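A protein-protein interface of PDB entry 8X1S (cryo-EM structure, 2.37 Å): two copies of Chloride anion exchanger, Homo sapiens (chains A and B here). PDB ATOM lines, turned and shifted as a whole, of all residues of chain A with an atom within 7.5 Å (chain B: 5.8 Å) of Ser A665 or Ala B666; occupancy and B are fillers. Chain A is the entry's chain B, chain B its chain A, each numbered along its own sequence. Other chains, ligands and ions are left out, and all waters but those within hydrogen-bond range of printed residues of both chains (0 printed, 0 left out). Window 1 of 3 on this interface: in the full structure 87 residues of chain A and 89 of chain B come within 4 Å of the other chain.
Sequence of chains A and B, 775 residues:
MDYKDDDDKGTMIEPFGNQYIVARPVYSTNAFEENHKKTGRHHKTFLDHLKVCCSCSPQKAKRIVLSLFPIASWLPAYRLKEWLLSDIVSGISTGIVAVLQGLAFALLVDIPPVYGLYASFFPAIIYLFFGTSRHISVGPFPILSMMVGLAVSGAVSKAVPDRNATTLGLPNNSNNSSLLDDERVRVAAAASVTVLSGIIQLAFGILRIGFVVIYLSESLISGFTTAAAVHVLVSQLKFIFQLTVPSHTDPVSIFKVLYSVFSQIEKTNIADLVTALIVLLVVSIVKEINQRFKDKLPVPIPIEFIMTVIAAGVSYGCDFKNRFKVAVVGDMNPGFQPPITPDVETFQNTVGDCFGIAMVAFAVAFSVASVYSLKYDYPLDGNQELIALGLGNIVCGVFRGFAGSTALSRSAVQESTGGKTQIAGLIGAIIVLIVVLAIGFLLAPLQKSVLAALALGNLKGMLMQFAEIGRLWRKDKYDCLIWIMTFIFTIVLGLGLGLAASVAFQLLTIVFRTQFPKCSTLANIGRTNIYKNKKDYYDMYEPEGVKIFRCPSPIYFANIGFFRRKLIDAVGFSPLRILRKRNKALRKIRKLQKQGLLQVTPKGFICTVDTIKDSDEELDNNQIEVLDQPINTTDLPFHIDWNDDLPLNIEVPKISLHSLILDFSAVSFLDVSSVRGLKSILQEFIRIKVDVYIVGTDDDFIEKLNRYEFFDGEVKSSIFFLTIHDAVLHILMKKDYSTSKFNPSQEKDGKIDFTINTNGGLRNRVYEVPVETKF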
ATOM      1  N   LEU A 522      -1.099 -20.303 -23.855  1.00  0.00           N
ATOM      2  CA  LEU A 522      -0.721 -19.994 -22.487  1.00  0.00           C
ATOM      3  C   LEU A 522       0.725 -20.309 -22.206  1.00  0.00           C
ATOM      4  O   LEU A 522       1.313 -21.178 -22.836  1.00  0.00           O
ATOM      5  CB  LEU A 522      -1.624 -20.733 -21.496  1.00  0.00           C
ATOM      6  CG  LEU A 522      -3.129 -20.547 -21.675  1.00  0.00           C
ATOM      7  CD1 LEU A 522      -3.884 -21.330 -20.615  1.00  0.00           C
ATOM      8  CD2 LEU A 522      -3.503 -19.076 -21.628  1.00  0.00           C
ATOM      9  N   ARG A 550      -6.031 -22.319 -25.161  1.00  0.00           N
ATOM     10  CA  ARG A 550      -7.234 -22.075 -24.382  1.00  0.00           C
ATOM     11  C   ARG A 550      -8.313 -21.492 -25.281  1.00  0.00           C
ATOM     12  O   ARG A 550      -8.061 -20.533 -26.017  1.00  0.00           O
ATOM     13  CB  ARG A 550      -6.939 -21.132 -23.221  1.00  0.00           C
ATOM     14  CG  ARG A 550      -8.146 -20.738 -22.442  1.00  0.00           C
ATOM     15  CD  ARG A 550      -7.798 -19.722 -21.399  1.00  0.00           C
ATOM     16  NE  ARG A 550      -8.990 -19.082 -20.862  1.00  0.00           N
ATOM     17  CZ  ARG A 550      -9.694 -19.551 -19.842  1.00  0.00           C
ATOM     18  NH1 ARG A 550     -10.764 -18.900 -19.424  1.00  0.00           N
ATOM     19  NH2 ARG A 550      -9.330 -20.669 -19.241  1.00  0.00           N
ATOM     20  N   CYS A 551      -9.504 -22.084 -25.226  1.00  0.00           N
ATOM     21  CA  CYS A 551     -10.711 -21.522 -25.812  1.00  0.00           C
ATOM     22  C   CYS A 551     -11.652 -21.136 -24.686  1.00  0.00           C
ATOM     23  O   CYS A 551     -12.112 -22.013 -23.948  1.00  0.00           O
ATOM     24  CB  CYS A 551     -11.390 -22.514 -26.751  1.00  0.00           C
ATOM     25  SG  CYS A 551     -12.835 -21.861 -27.606  1.00  0.00           S
ATOM     26  N   PRO A 552     -11.941 -19.868 -24.507  1.00  0.00           N
ATOM     27  CA  PRO A 552     -12.720 -19.421 -23.343  1.00  0.00           C
ATOM     28  C   PRO A 552     -14.222 -19.404 -23.576  1.00  0.00           C
ATOM     29  O   PRO A 552     -14.907 -18.424 -23.286  1.00  0.00           O
ATOM     30  CB  PRO A 552     -12.180 -17.992 -23.135  1.00  0.00           C
ATOM     31  CG  PRO A 552     -11.912 -17.538 -24.525  1.00  0.00           C
ATOM     32  CD  PRO A 552     -11.534 -18.740 -25.350  1.00  0.00           C
ATOM     33  N   SER A 553     -14.709 -20.499 -24.113  1.00  0.00           N
ATOM     34  CA  SER A 553     -16.085 -20.585 -24.471  1.00  0.00           C
ATOM     35  C   SER A 553     -16.469 -22.020 -24.636  1.00  0.00           C
ATOM     36  O   SER A 553     -15.615 -22.875 -24.789  1.00  0.00           O
ATOM     37  CB  SER A 553     -16.235 -19.879 -25.822  1.00  0.00           C
ATOM     38  OG  SER A 553     -17.569 -19.724 -26.212  1.00  0.00           O
ATOM     39  N   PRO A 554     -17.770 -22.305 -24.567  1.00  0.00           N
ATOM     40  CA  PRO A 554     -18.185 -23.668 -24.874  1.00  0.00           C
ATOM     41  C   PRO A 554     -18.046 -23.828 -26.382  1.00  0.00           C
ATOM     42  O   PRO A 554     -18.286 -22.901 -27.131  1.00  0.00           O
ATOM     43  CB  PRO A 554     -19.659 -23.685 -24.485  1.00  0.00           C
ATOM     44  CG  PRO A 554     -20.066 -22.262 -24.393  1.00  0.00           C
ATOM     45  CD  PRO A 554     -18.852 -21.521 -23.960  1.00  0.00           C
ATOM     46  N   LEU A 662      -4.887 -28.764 -24.183  1.00  0.00           N
ATOM     47  CA  LEU A 662      -6.095 -27.991 -24.426  1.00  0.00           C
ATOM     48  C   LEU A 662      -6.712 -27.637 -23.083  1.00  0.00           C
ATOM     49  O   LEU A 662      -7.198 -28.513 -22.368  1.00  0.00           O
ATOM     50  CB  LEU A 662      -7.076 -28.770 -25.294  1.00  0.00           C
ATOM     51  CG  LEU A 662      -6.612 -29.087 -26.713  1.00  0.00           C
ATOM     52  CD1 LEU A 662      -7.673 -29.861 -27.446  1.00  0.00           C
ATOM     53  CD2 LEU A 662      -6.266 -27.825 -27.462  1.00  0.00           C
ATOM     54  N   ASP A 663      -6.683 -26.357 -22.741  1.00  0.00           N
ATOM     55  CA  ASP A 663      -7.273 -25.865 -21.503  1.00  0.00           C
ATOM     56  C   ASP A 663      -8.771 -25.709 -21.713  1.00  0.00           C
ATOM     57  O   ASP A 663      -9.227 -24.762 -22.352  1.00  0.00           O
ATOM     58  CB  ASP A 663      -6.625 -24.552 -21.091  1.00  0.00           C
ATOM     59  CG  ASP A 663      -7.286 -23.933 -19.890  1.00  0.00           C
ATOM     60  OD1 ASP A 663      -7.665 -24.677 -18.968  1.00  0.00           O
ATOM     61  OD2 ASP A 663      -7.422 -22.699 -19.859  1.00  0.00           O
ATOM     62  N   PHE A 664      -9.547 -26.643 -21.170  1.00  0.00           N
ATOM     63  CA  PHE A 664     -10.982 -26.707 -21.397  1.00  0.00           C
ATOM     64  C   PHE A 664     -11.786 -26.285 -20.175  1.00  0.00           C
ATOM     65  O   PHE A 664     -12.916 -26.739 -19.997  1.00  0.00           O
ATOM     66  CB  PHE A 664     -11.381 -28.118 -21.820  1.00  0.00           C
ATOM     67  CG  PHE A 664     -11.453 -28.316 -23.298  1.00  0.00           C
ATOM     68  CD1 PHE A 664     -10.659 -27.586 -24.150  1.00  0.00           C
ATOM     69  CD2 PHE A 664     -12.320 -29.239 -23.834  1.00  0.00           C
ATOM     70  CE1 PHE A 664     -10.728 -27.774 -25.501  1.00  0.00           C
ATOM     71  CE2 PHE A 664     -12.393 -29.426 -25.186  1.00  0.00           C
ATOM     72  CZ  PHE A 664     -11.595 -28.693 -26.017  1.00  0.00           C
ATOM     73  N   SER A 665     -11.229 -25.424 -19.329  1.00  0.00           N
ATOM     74  CA  SER A 665     -11.925 -25.053 -18.103  1.00  0.00           C
ATOM     75  C   SER A 665     -13.154 -24.205 -18.388  1.00  0.00           C
ATOM     76  O   SER A 665     -14.180 -24.353 -17.721  1.00  0.00           O
ATOM     77  CB  SER A 665     -10.980 -24.320 -17.161  1.00  0.00           C
ATOM     78  OG  SER A 665     -10.094 -23.500 -17.882  1.00  0.00           O
ATOM     79  N   ALA A 666     -13.073 -23.318 -19.371  1.00  0.00           N
ATOM     80  CA  ALA A 666     -14.181 -22.444 -19.716  1.00  0.00           C
ATOM     81  C   ALA A 666     -15.082 -23.021 -20.794  1.00  0.00           C
ATOM     82  O   ALA A 666     -16.047 -22.366 -21.183  1.00  0.00           O
ATOM     83  CB  ALA A 666     -13.656 -21.081 -20.162  1.00  0.00           C
ATOM     84  N   VAL A 667     -14.794 -24.223 -21.285  1.00  0.00           N
ATOM     85  CA  VAL A 667     -15.641 -24.891 -22.268  1.00  0.00           C
ATOM     86  C   VAL A 667     -16.800 -25.518 -21.502  1.00  0.00           C
ATOM     87  O   VAL A 667     -16.682 -26.615 -20.966  1.00  0.00           O
ATOM     88  CB  VAL A 667     -14.865 -25.927 -23.081  1.00  0.00           C
ATOM     89  CG1 VAL A 667     -15.770 -26.600 -24.082  1.00  0.00           C
ATOM     90  CG2 VAL A 667     -13.700 -25.270 -23.781  1.00  0.00           C
ATOM     91  N   SER A 668     -17.880 -24.781 -21.351  1.00  0.00           N
ATOM     92  CA  SER A 668     -19.009 -25.256 -20.573  1.00  0.00           C
ATOM     93  C   SER A 668     -19.644 -26.541 -21.079  1.00  0.00           C
ATOM     94  O   SER A 668     -19.868 -27.468 -20.327  1.00  0.00           O
ATOM     95  CB  SER A 668     -20.051 -24.152 -20.462  1.00  0.00           C
ATOM     96  OG  SER A 668     -19.445 -22.976 -19.985  1.00  0.00           O
ATOM     97  N   PHE A 669     -19.939 -26.577 -22.363  1.00  0.00           N
ATOM     98  CA  PHE A 669     -20.575 -27.716 -22.974  1.00  0.00           C
ATOM     99  C   PHE A 669     -20.025 -27.946 -24.356  1.00  0.00           C
ATOM    100  O   PHE A 669     -19.311 -27.129 -24.884  1.00  0.00           O
ATOM    101  CB  PHE A 669     -22.103 -27.522 -23.043  1.00  0.00           C
ATOM    102  CG  PHE A 669     -22.543 -26.397 -23.939  1.00  0.00           C
ATOM    103  CD1 PHE A 669     -22.704 -26.600 -25.296  1.00  0.00           C
ATOM    104  CD2 PHE A 669     -22.804 -25.144 -23.423  1.00  0.00           C
ATOM    105  CE1 PHE A 669     -23.095 -25.574 -26.119  1.00  0.00           C
ATOM    106  CE2 PHE A 669     -23.205 -24.113 -24.242  1.00  0.00           C
ATOM    107  CZ  PHE A 669     -23.353 -24.329 -25.593  1.00  0.00           C
ATOM    108  N   ILE A 694      -6.209 -32.918 -22.348  1.00  0.00           N
ATOM    109  CA  ILE A 694      -7.332 -32.040 -22.097  1.00  0.00           C
ATOM    110  C   ILE A 694      -7.348 -31.841 -20.596  1.00  0.00           C
ATOM    111  O   ILE A 694      -7.338 -32.795 -19.856  1.00  0.00           O
ATOM    112  CB  ILE A 694      -8.640 -32.619 -22.651  1.00  0.00           C
ATOM    113  CG1 ILE A 694      -8.489 -32.871 -24.151  1.00  0.00           C
ATOM    114  CG2 ILE A 694      -9.797 -31.673 -22.383  1.00  0.00           C
ATOM    115  CD1 ILE A 694      -9.765 -33.212 -24.868  1.00  0.00           C
ATOM    116  N   VAL A 695      -7.322 -30.594 -20.140  1.00  0.00           N
ATOM    117  CA  VAL A 695      -7.235 -30.316 -18.717  1.00  0.00           C
ATOM    118  C   VAL A 695      -8.346 -29.359 -18.325  1.00  0.00           C
ATOM    119  O   VAL A 695      -8.939 -28.678 -19.159  1.00  0.00           O
ATOM    120  CB  VAL A 695      -5.865 -29.737 -18.326  1.00  0.00           C
ATOM    121  CG1 VAL A 695      -4.763 -30.670 -18.751  1.00  0.00           C
ATOM    122  CG2 VAL A 695      -5.679 -28.378 -18.948  1.00  0.00           C
ATOM    123  N   GLY A 696      -8.636 -29.330 -17.031  1.00  0.00           N
ATOM    124  CA  GLY A 696      -9.504 -28.324 -16.468  1.00  0.00           C
ATOM    125  C   GLY A 696     -10.985 -28.586 -16.565  1.00  0.00           C
ATOM    126  O   GLY A 696     -11.771 -27.678 -16.291  1.00  0.00           O
ATOM    127  N   THR A 697     -11.399 -29.786 -16.940  1.00  0.00           N
ATOM    128  CA  THR A 697     -12.811 -30.116 -17.028  1.00  0.00           C
ATOM    129  C   THR A 697     -13.274 -30.777 -15.738  1.00  0.00           C
ATOM    130  O   THR A 697     -12.468 -31.264 -14.945  1.00  0.00           O
ATOM    131  CB  THR A 697     -13.074 -31.039 -18.214  1.00  0.00           C
ATOM    132  OG1 THR A 697     -12.481 -32.313 -17.967  1.00  0.00           O
ATOM    133  CG2 THR A 697     -12.470 -30.468 -19.460  1.00  0.00           C
ATOM    134  N   ASP A 698     -14.585 -30.767 -15.522  1.00  0.00           N
ATOM    135  CA  ASP A 698     -15.159 -31.472 -14.388  1.00  0.00           C
ATOM    136  C   ASP A 698     -15.638 -32.859 -14.814  1.00  0.00           C
ATOM    137  O   ASP A 698     -15.504 -33.268 -15.968  1.00  0.00           O
ATOM    138  CB  ASP A 698     -16.285 -30.655 -13.762  1.00  0.00           C
ATOM    139  CG  ASP A 698     -17.356 -30.281 -14.755  1.00  0.00           C
ATOM    140  OD1 ASP A 698     -18.548 -30.320 -14.392  1.00  0.00           O
ATOM    141  OD2 ASP A 698     -17.002 -29.946 -15.903  1.00  0.00           O
ATOM    142  N   PHE A 701     -18.464 -33.385 -17.377  1.00  0.00           N
ATOM    143  CA  PHE A 701     -17.986 -33.198 -18.738  1.00  0.00           C
ATOM    144  C   PHE A 701     -17.545 -34.518 -19.353  1.00  0.00           C
ATOM    145  O   PHE A 701     -17.892 -34.830 -20.496  1.00  0.00           O
ATOM    146  CB  PHE A 701     -16.842 -32.186 -18.728  1.00  0.00           C
ATOM    147  CG  PHE A 701     -16.464 -31.671 -20.081  1.00  0.00           C
ATOM    148  CD1 PHE A 701     -15.512 -32.320 -20.839  1.00  0.00           C
ATOM    149  CD2 PHE A 701     -17.045 -30.525 -20.585  1.00  0.00           C
ATOM    150  CE1 PHE A 701     -15.163 -31.848 -22.071  1.00  0.00           C
ATOM    151  CE2 PHE A 701     -16.694 -30.049 -21.820  1.00  0.00           C
ATOM    152  CZ  PHE A 701     -15.750 -30.710 -22.559  1.00  0.00           C
ATOM    153  N   LEU A 722      -5.940 -33.210 -14.540  1.00  0.00           N
ATOM    154  CA  LEU A 722      -6.648 -32.318 -13.636  1.00  0.00           C
ATOM    155  C   LEU A 722      -6.445 -30.862 -14.025  1.00  0.00           C
ATOM    156  O   LEU A 722      -7.410 -30.121 -14.223  1.00  0.00           O
ATOM    157  CB  LEU A 722      -6.199 -32.563 -12.199  1.00  0.00           C
ATOM    158  CG  LEU A 722      -6.710 -33.825 -11.514  1.00  0.00           C
ATOM    159  CD1 LEU A 722      -6.553 -33.690 -10.028  1.00  0.00           C
ATOM    160  CD2 LEU A 722      -8.148 -34.083 -11.868  1.00  0.00           C
ATOM    161  N   ILE A 724      -3.467 -27.734 -15.864  1.00  0.00           N
ATOM    162  CA  ILE A 724      -2.401 -27.538 -16.837  1.00  0.00           C
ATOM    163  C   ILE A 724      -1.073 -28.006 -16.274  1.00  0.00           C
ATOM    164  O   ILE A 724      -0.255 -28.587 -16.989  1.00  0.00           O
ATOM    165  CB  ILE A 724      -2.324 -26.063 -17.271  1.00  0.00           C
ATOM    166  CG1 ILE A 724      -3.645 -25.593 -17.855  1.00  0.00           C
ATOM    167  CG2 ILE A 724      -1.226 -25.859 -18.279  1.00  0.00           C
ATOM    168  CD1 ILE A 724      -3.676 -24.133 -18.140  1.00  0.00           C
ATOM    169  N   ARG B 550     -19.947 -23.521  -7.370  1.00  0.00           N
ATOM    170  CA  ARG B 550     -19.553 -23.553  -8.769  1.00  0.00           C
ATOM    171  C   ARG B 550     -20.794 -23.532  -9.647  1.00  0.00           C
ATOM    172  O   ARG B 550     -21.724 -24.315  -9.432  1.00  0.00           O
ATOM    173  CB  ARG B 550     -18.713 -24.790  -9.061  1.00  0.00           C
ATOM    174  CG  ARG B 550     -18.367 -24.958 -10.501  1.00  0.00           C
ATOM    175  CD  ARG B 550     -17.647 -26.250 -10.728  1.00  0.00           C
ATOM    176  NE  ARG B 550     -17.601 -26.592 -12.142  1.00  0.00           N
ATOM    177  CZ  ARG B 550     -16.655 -26.184 -12.978  1.00  0.00           C
ATOM    178  NH1 ARG B 550     -16.695 -26.544 -14.247  1.00  0.00           N
ATOM    179  NH2 ARG B 550     -15.671 -25.417 -12.545  1.00  0.00           N
ATOM    180  N   CYS B 551     -20.807 -22.626 -10.622  1.00  0.00           N
ATOM    181  CA  CYS B 551     -21.778 -22.620 -11.705  1.00  0.00           C
ATOM    182  C   CYS B 551     -21.052 -22.949 -12.997  1.00  0.00           C
ATOM    183  O   CYS B 551     -20.191 -22.174 -13.426  1.00  0.00           O
ATOM    184  CB  CYS B 551     -22.479 -21.270 -11.819  1.00  0.00           C
ATOM    185  SG  CYS B 551     -23.777 -21.209 -13.067  1.00  0.00           S
ATOM    186  N   PRO B 552     -21.246 -24.158 -13.516  1.00  0.00           N
ATOM    187  CA  PRO B 552     -20.468 -24.594 -14.675  1.00  0.00           C
ATOM    188  C   PRO B 552     -20.976 -24.068 -15.993  1.00  0.00           C
ATOM    189  O   PRO B 552     -21.003 -24.793 -16.965  1.00  0.00           O
ATOM    190  CB  PRO B 552     -20.650 -26.097 -14.624  1.00  0.00           C
ATOM    191  CG  PRO B 552     -22.036 -26.259 -14.106  1.00  0.00           C
ATOM    192  CD  PRO B 552     -22.330 -25.101 -13.203  1.00  0.00           C
ATOM    193  N   SER B 553     -21.312 -22.798 -16.037  1.00  0.00           N
ATOM    194  CA  SER B 553     -21.883 -22.239 -17.225  1.00  0.00           C
ATOM    195  C   SER B 553     -21.731 -20.743 -17.210  1.00  0.00           C
ATOM    196  O   SER B 553     -21.475 -20.170 -16.167  1.00  0.00           O
ATOM    197  CB  SER B 553     -23.366 -22.617 -17.197  1.00  0.00           C
ATOM    198  OG  SER B 553     -24.088 -22.165 -18.309  1.00  0.00           O
ATOM    199  N   PRO B 554     -21.828 -20.097 -18.378  1.00  0.00           N
ATOM    200  CA  PRO B 554     -21.811 -18.636 -18.363  1.00  0.00           C
ATOM    201  C   PRO B 554     -23.130 -18.163 -17.764  1.00  0.00           C
ATOM    202  O   PRO B 554     -24.157 -18.777 -17.970  1.00  0.00           O
ATOM    203  CB  PRO B 554     -21.745 -18.263 -19.841  1.00  0.00           C
ATOM    204  CG  PRO B 554     -22.154 -19.482 -20.578  1.00  0.00           C
ATOM    205  CD  PRO B 554     -21.726 -20.635 -19.740  1.00  0.00           C
ATOM    206  N   ASP B 663     -16.575 -20.188  -7.701  1.00  0.00           N
ATOM    207  CA  ASP B 663     -15.705 -20.751  -8.726  1.00  0.00           C
ATOM    208  C   ASP B 663     -16.262 -20.372 -10.089  1.00  0.00           C
ATOM    209  O   ASP B 663     -17.247 -20.945 -10.553  1.00  0.00           O
ATOM    210  CB  ASP B 663     -15.600 -22.260  -8.564  1.00  0.00           C
ATOM    211  CG  ASP B 663     -14.821 -22.908  -9.675  1.00  0.00           C
ATOM    212  OD1 ASP B 663     -13.812 -22.327 -10.113  1.00  0.00           O
ATOM    213  OD2 ASP B 663     -15.208 -24.006 -10.108  1.00  0.00           O
ATOM    214  N   PHE B 664     -15.628 -19.400 -10.739  1.00  0.00           N
ATOM    215  CA  PHE B 664     -16.119 -18.835 -11.987  1.00  0.00           C
ATOM    216  C   PHE B 664     -15.287 -19.260 -13.187  1.00  0.00           C
ATOM    217  O   PHE B 664     -15.216 -18.531 -14.176  1.00  0.00           O
ATOM    218  CB  PHE B 664     -16.152 -17.312 -11.891  1.00  0.00           C
ATOM    219  CG  PHE B 664     -17.473 -16.752 -11.480  1.00  0.00           C
ATOM    220  CD1 PHE B 664     -18.325 -17.468 -10.673  1.00  0.00           C
ATOM    221  CD2 PHE B 664     -17.863 -15.502 -11.905  1.00  0.00           C
ATOM    222  CE1 PHE B 664     -19.531 -16.951 -10.299  1.00  0.00           C
ATOM    223  CE2 PHE B 664     -19.070 -14.984 -11.531  1.00  0.00           C
ATOM    224  CZ  PHE B 664     -19.903 -15.708 -10.728  1.00  0.00           C
ATOM    225  N   SER B 665     -14.657 -20.431 -13.126  1.00  0.00           N
ATOM    226  CA  SER B 665     -13.783 -20.845 -14.217  1.00  0.00           C
ATOM    227  C   SER B 665     -14.571 -21.168 -15.476  1.00  0.00           C
ATOM    228  O   SER B 665     -14.122 -20.869 -16.585  1.00  0.00           O
ATOM    229  CB  SER B 665     -12.944 -22.042 -13.793  1.00  0.00           C
ATOM    230  OG  SER B 665     -13.684 -22.902 -12.963  1.00  0.00           O
ATOM    231  N   ALA B 666     -15.743 -21.772 -15.331  1.00  0.00           N
ATOM    232  CA  ALA B 666     -16.568 -22.143 -16.467  1.00  0.00           C
ATOM    233  C   ALA B 666     -17.574 -21.070 -16.847  1.00  0.00           C
ATOM    234  O   ALA B 666     -18.342 -21.274 -17.787  1.00  0.00           O
ATOM    235  CB  ALA B 666     -17.299 -23.452 -16.182  1.00  0.00           C
ATOM    236  N   VAL B 667     -17.591 -19.939 -16.148  1.00  0.00           N
ATOM    237  CA  VAL B 667     -18.469 -18.823 -16.485  1.00  0.00           C
ATOM    238  C   VAL B 667     -17.806 -18.066 -17.628  1.00  0.00           C
ATOM    239  O   VAL B 667     -16.940 -17.225 -17.409  1.00  0.00           O
ATOM    240  CB  VAL B 667     -18.735 -17.922 -15.279  1.00  0.00           C
ATOM    241  CG1 VAL B 667     -19.640 -16.777 -15.663  1.00  0.00           C
ATOM    242  CG2 VAL B 667     -19.346 -18.725 -14.156  1.00  0.00           C
ATOM    243  N   SER B 668     -18.215 -18.370 -18.857  1.00  0.00           N
ATOM    244  CA  SER B 668     -17.546 -17.846 -20.041  1.00  0.00           C
ATOM    245  C   SER B 668     -17.754 -16.344 -20.187  1.00  0.00           C
ATOM    246  O   SER B 668     -16.805 -15.596 -20.424  1.00  0.00           O
ATOM    247  CB  SER B 668     -18.051 -18.577 -21.284  1.00  0.00           C
ATOM    248  OG  SER B 668     -17.802 -19.962 -21.185  1.00  0.00           O
ATOM    249  N   GLY B 696     -10.762 -18.212 -10.450  1.00  0.00           N
ATOM    250  CA  GLY B 696     -10.736 -18.998 -11.662  1.00  0.00           C
ATOM    251  C   GLY B 696     -11.054 -18.266 -12.941  1.00  0.00           C
ATOM    252  O   GLY B 696     -11.250 -18.919 -13.967  1.00  0.00           O
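The guanidinium group (NH1) of Arg B550 is in salt-bridge range of the side-chain carboxylate (OD2) of Asp A698 (3.8 Å). O of Ala B666 sits at hydrogen-bond distance from OG of Ser A668. The side-chain hydroxyl (OG) of Ser B668 lies within hydrogen-bond range of the backbone carbonyl oxygen (O) of Ala A666, 3.0 Å away.
The guanidinium group of Arg B550 lies within salt-bridge range of the side-chain carboxylate of Asp B663 (2.9 Å). The side-chain hydroxyl (OG) of Ser A665 sits at hydrogen-bond distance from the guanidinium group (NH2) of Arg A550 (3.2 Å). The side-chain hydroxyl (OG) of Ser B665 sits at hydrogen-bond distance from the side-chain carboxylate (OD1) of Asp B663, at 2.9 Å. The side-chain hydroxyl of Ser A665 is in hydrogen-bond range of the side-chain carboxylate of Asp A663 (2.9 Å). OG of Ser B665 sits at hydrogen-bond distance from NH2 of Arg B550.
Pro A552 touches Ser B668 (O to CB, 3.7 Å). Ser A553 touches Ser B668 (CA to OG, 3.8 Å). Pro A554 touches Ser B668 (CD to OG, 3.4 Å). O of Ser A665 touches O of Ser B665, 3.7 Å away. Ser A665 touches Ala B666. O of Ser B665 touches CA of Ala A666 (3.5 Å). Pro B552 touches Ser A668. OG of Ser A668 touches CA of Ser B553, 3.8 Å away. Ser A668 touches Pro B554. Ser A668 touches Ser B668.
Of the printed residues of chain B, Ser A553 touches Ser B668 (3.8 Å). Printed residues of chain B within 4 Å of Pro A554: Ser B668 (3.4 Å). Ser A665 touches just these residues of chain B: Ser B665 (3.7 Å) and Ala B666 (3.5 Å). Val A695 touches none of the printed residues of chain B. Of the printed residues of chain A, Ser B553 touches Ser A668 (3.8 Å). Printed residues of chain A within 4 Å of Ala B666: Ser A665 and Ser A668. Of the printed residues of chain A, Ser B668 touches Pro A552, Ser A553, Pro A554, Ala A666 and Ser A668. The nearest printed residue of chain A that does not touch Arg B550 is Ser A665 (4.8 Å).
Hydrophobic or aromatic side chains of chain B within 4 Å of the printed part of chain A: Pro B554 and Ala B666. Hydrophobic or aromatic side chains of chain A within 4 Å of the printed part of chain B: Pro A554 and Ala A666. Among the printed residues, 13 pairs touch across the chains.
Pro A554 touches Ser B668, and with the chains exchanged Ser A668 touches Pro B554. Ser A665 touches its own counterpart, Ser B665. Ser A665 touches Ala B666, and with the chains exchanged Ala A666 touches Ser B665. Ser B668 touches its own counterpart, Ser A668. Of the 13 pairs that touch across the chains among the printed residues, 12 have their exchanged pair printed and touching as well.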
